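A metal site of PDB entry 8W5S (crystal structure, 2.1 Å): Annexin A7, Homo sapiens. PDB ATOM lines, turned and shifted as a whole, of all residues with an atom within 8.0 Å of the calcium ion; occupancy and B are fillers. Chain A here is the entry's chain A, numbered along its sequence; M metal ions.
Of the 14 residues printed, 4 come within 4 Å of the calcium ion.
The nearest printed residue that does not touch the calcium ion is Lys 243 (4.3 Å).
The backbone carbonyl oxygen (O) of Asp 286 is in hydrogen-bond range of the side-chain hydroxyl (OG1) of Thr 247, 3.2 Å away.
The calcium ion is bound by O of Met 242 (2.3 Å), OD1 of Asp 286 (2.3 Å), O of Gly 244 (2.4 Å), O of Gly 246 (2.7 Å) and OD2 of Asp 286 (2.7 Å).
The calcium ion has five donor atoms within binding distance.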
ATOM      1  N   TYR A 239       9.391  -8.990  21.597  1.00  0.00           N
ATOM      2  CA  TYR A 239       9.832  -7.974  20.641  1.00  0.00           C
ATOM      3  C   TYR A 239       9.768  -8.498  19.212  1.00  0.00           C
ATOM      4  O   TYR A 239       9.260  -7.823  18.317  1.00  0.00           O
ATOM      5  CB  TYR A 239      11.250  -7.518  20.989  1.00  0.00           C
ATOM      6  CG  TYR A 239      11.865  -6.570  19.994  1.00  0.00           C
ATOM      7  CD1 TYR A 239      11.604  -5.211  20.049  1.00  0.00           C
ATOM      8  CD2 TYR A 239      12.737  -7.031  19.020  1.00  0.00           C
ATOM      9  CE1 TYR A 239      12.173  -4.344  19.133  1.00  0.00           C
ATOM     10  CE2 TYR A 239      13.310  -6.172  18.109  1.00  0.00           C
ATOM     11  CZ  TYR A 239      13.027  -4.829  18.177  1.00  0.00           C
ATOM     12  OH  TYR A 239      13.601  -3.965  17.274  1.00  0.00           O
ATOM     13  N   TYR A 240      10.280  -9.712  19.002  1.00  0.00           N
ATOM     14  CA  TYR A 240      10.208 -10.335  17.678  1.00  0.00           C
ATOM     15  C   TYR A 240       8.768 -10.505  17.215  1.00  0.00           C
ATOM     16  O   TYR A 240       8.492 -10.440  16.010  1.00  0.00           O
ATOM     17  CB  TYR A 240      10.889 -11.704  17.703  1.00  0.00           C
ATOM     18  CG  TYR A 240      12.398 -11.693  17.648  1.00  0.00           C
ATOM     19  CD1 TYR A 240      13.098 -10.699  16.985  1.00  0.00           C
ATOM     20  CD2 TYR A 240      13.127 -12.706  18.254  1.00  0.00           C
ATOM     21  CE1 TYR A 240      14.491 -10.709  16.929  1.00  0.00           C
ATOM     22  CE2 TYR A 240      14.508 -12.725  18.217  1.00  0.00           C
ATOM     23  CZ  TYR A 240      15.186 -11.728  17.556  1.00  0.00           C
ATOM     24  OH  TYR A 240      16.560 -11.763  17.519  1.00  0.00           O
ATOM     25  N   ALA A 241       7.847 -10.722  18.147  1.00  0.00           N
ATOM     26  CA  ALA A 241       6.476 -11.065  17.783  1.00  0.00           C
ATOM     27  C   ALA A 241       5.763  -9.891  17.116  1.00  0.00           C
ATOM     28  O   ALA A 241       4.977 -10.081  16.178  1.00  0.00           O
ATOM     29  CB  ALA A 241       5.701 -11.539  19.013  1.00  0.00           C
ATOM     30  N   MET A 242       6.038  -8.668  17.572  1.00  0.00           N
ATOM     31  CA  MET A 242       5.357  -7.493  17.051  1.00  0.00           C
ATOM     32  C   MET A 242       6.212  -6.660  16.101  1.00  0.00           C
ATOM     33  O   MET A 242       5.716  -5.649  15.582  1.00  0.00           O
ATOM     34  CB  MET A 242       4.859  -6.605  18.198  1.00  0.00           C
ATOM     35  CG  MET A 242       4.404  -7.361  19.426  1.00  0.00           C
ATOM     36  SD  MET A 242       4.062  -6.266  20.811  1.00  0.00           S
ATOM     37  CE  MET A 242       5.073  -7.012  22.075  1.00  0.00           C
ATOM     38  N   LYS A 243       7.464  -7.037  15.863  1.00  0.00           N
ATOM     39  CA  LYS A 243       8.301  -6.280  14.949  1.00  0.00           C
ATOM     40  C   LYS A 243       8.071  -6.742  13.515  1.00  0.00           C
ATOM     41  O   LYS A 243       7.949  -7.942  13.251  1.00  0.00           O
ATOM     42  CB  LYS A 243       9.778  -6.386  15.309  1.00  0.00           C
ATOM     43  CG  LYS A 243      10.520  -5.124  14.927  1.00  0.00           C
ATOM     44  CD  LYS A 243      11.939  -5.346  14.462  1.00  0.00           C
ATOM     45  CE  LYS A 243      12.354  -4.203  13.543  1.00  0.00           C
ATOM     46  NZ  LYS A 243      12.592  -2.922  14.277  1.00  0.00           N
ATOM     47  N   GLY A 244       8.025  -5.786  12.604  1.00  0.00           N
ATOM     48  CA  GLY A 244       7.556  -6.019  11.256  1.00  0.00           C
ATOM     49  C   GLY A 244       6.099  -5.617  11.108  1.00  0.00           C
ATOM     50  O   GLY A 244       5.445  -5.150  12.049  1.00  0.00           O
ATOM     51  N   ALA A 245       5.583  -5.817   9.902  1.00  0.00           N
ATOM     52  CA  ALA A 245       4.178  -5.526   9.622  1.00  0.00           C
ATOM     53  C   ALA A 245       3.322  -6.655  10.169  1.00  0.00           C
ATOM     54  O   ALA A 245       3.490  -7.815   9.793  1.00  0.00           O
ATOM     55  CB  ALA A 245       3.958  -5.344   8.127  1.00  0.00           C
ATOM     56  N   GLY A 246       2.387  -6.318  11.051  1.00  0.00           N
ATOM     57  CA  GLY A 246       1.534  -7.321  11.654  1.00  0.00           C
ATOM     58  C   GLY A 246       2.064  -7.793  12.990  1.00  0.00           C
ATOM     59  O   GLY A 246       3.046  -7.273  13.535  1.00  0.00           O
ATOM     60  N   THR A 247       1.398  -8.816  13.511  1.00  0.00           N
ATOM     61  CA  THR A 247       1.746  -9.381  14.817  1.00  0.00           C
ATOM     62  C   THR A 247       1.704 -10.897  14.747  1.00  0.00           C
ATOM     63  O   THR A 247       0.838 -11.482  14.101  1.00  0.00           O
ATOM     64  CB  THR A 247       0.800  -8.894  15.918  1.00  0.00           C
ATOM     65  OG1 THR A 247       0.725  -7.467  15.899  1.00  0.00           O
ATOM     66  CG2 THR A 247       1.277  -9.361  17.296  1.00  0.00           C
ATOM     67  N   ASP A 248       2.671 -11.531  15.415  1.00  0.00           N
ATOM     68  CA  ASP A 248       2.598 -12.962  15.722  1.00  0.00           C
ATOM     69  C   ASP A 248       1.712 -13.073  16.961  1.00  0.00           C
ATOM     70  O   ASP A 248       2.197 -13.068  18.098  1.00  0.00           O
ATOM     71  CB  ASP A 248       3.984 -13.547  15.943  1.00  0.00           C
ATOM     72  CG  ASP A 248       3.951 -15.036  16.218  1.00  0.00           C
ATOM     73  OD1 ASP A 248       2.881 -15.653  16.110  1.00  0.00           O
ATOM     74  OD2 ASP A 248       5.027 -15.596  16.554  1.00  0.00           O
ATOM     75  N   MET A 282       4.855  -0.948  22.642  1.00  0.00           N
ATOM     76  CA  MET A 282       4.939  -1.855  21.501  1.00  0.00           C
ATOM     77  C   MET A 282       3.583  -2.504  21.219  1.00  0.00           C
ATOM     78  O   MET A 282       3.149  -2.590  20.061  1.00  0.00           O
ATOM     79  CB  MET A 282       6.001  -2.922  21.759  1.00  0.00           C
ATOM     80  CG  MET A 282       6.409  -3.724  20.532  1.00  0.00           C
ATOM     81  SD  MET A 282       7.901  -3.130  19.720  1.00  0.00           S
ATOM     82  CE  MET A 282       7.949  -4.200  18.282  1.00  0.00           C
ATOM     83  N   GLY A 285       0.770  -0.110  19.837  1.00  0.00           N
ATOM     84  CA  GLY A 285       0.916   0.172  18.426  1.00  0.00           C
ATOM     85  C   GLY A 285       0.573  -0.996  17.530  1.00  0.00           C
ATOM     86  O   GLY A 285       0.164  -0.800  16.378  1.00  0.00           O
ATOM     87  N   ASP A 286       0.688  -2.226  18.036  1.00  0.00           N
ATOM     88  CA  ASP A 286       0.547  -3.414  17.219  1.00  0.00           C
ATOM     89  C   ASP A 286      -0.820  -4.075  17.320  1.00  0.00           C
ATOM     90  O   ASP A 286      -1.129  -4.945  16.501  1.00  0.00           O
ATOM     91  CB  ASP A 286       1.626  -4.441  17.591  1.00  0.00           C
ATOM     92  CG  ASP A 286       2.528  -4.781  16.436  1.00  0.00           C
ATOM     93  OD1 ASP A 286       3.225  -3.884  15.924  1.00  0.00           O
ATOM     94  OD2 ASP A 286       2.553  -5.975  16.036  1.00  0.00           O
ATOM     95  N   THR A 287      -1.639  -3.706  18.302  1.00  0.00           N
ATOM     96  CA  THR A 287      -2.937  -4.329  18.533  1.00  0.00           C
ATOM     97  C   THR A 287      -4.019  -3.252  18.590  1.00  0.00           C
ATOM     98  O   THR A 287      -3.739  -2.062  18.700  1.00  0.00           O
ATOM     99  CB  THR A 287      -2.945  -5.166  19.819  1.00  0.00           C
ATOM    100  OG1 THR A 287      -2.760  -4.313  20.952  1.00  0.00           O
ATOM    101  CG2 THR A 287      -1.828  -6.210  19.795  1.00  0.00           C
HETATM  102 CA    CA M   1       4.154  -4.916  14.076  1.00  0.00          CA
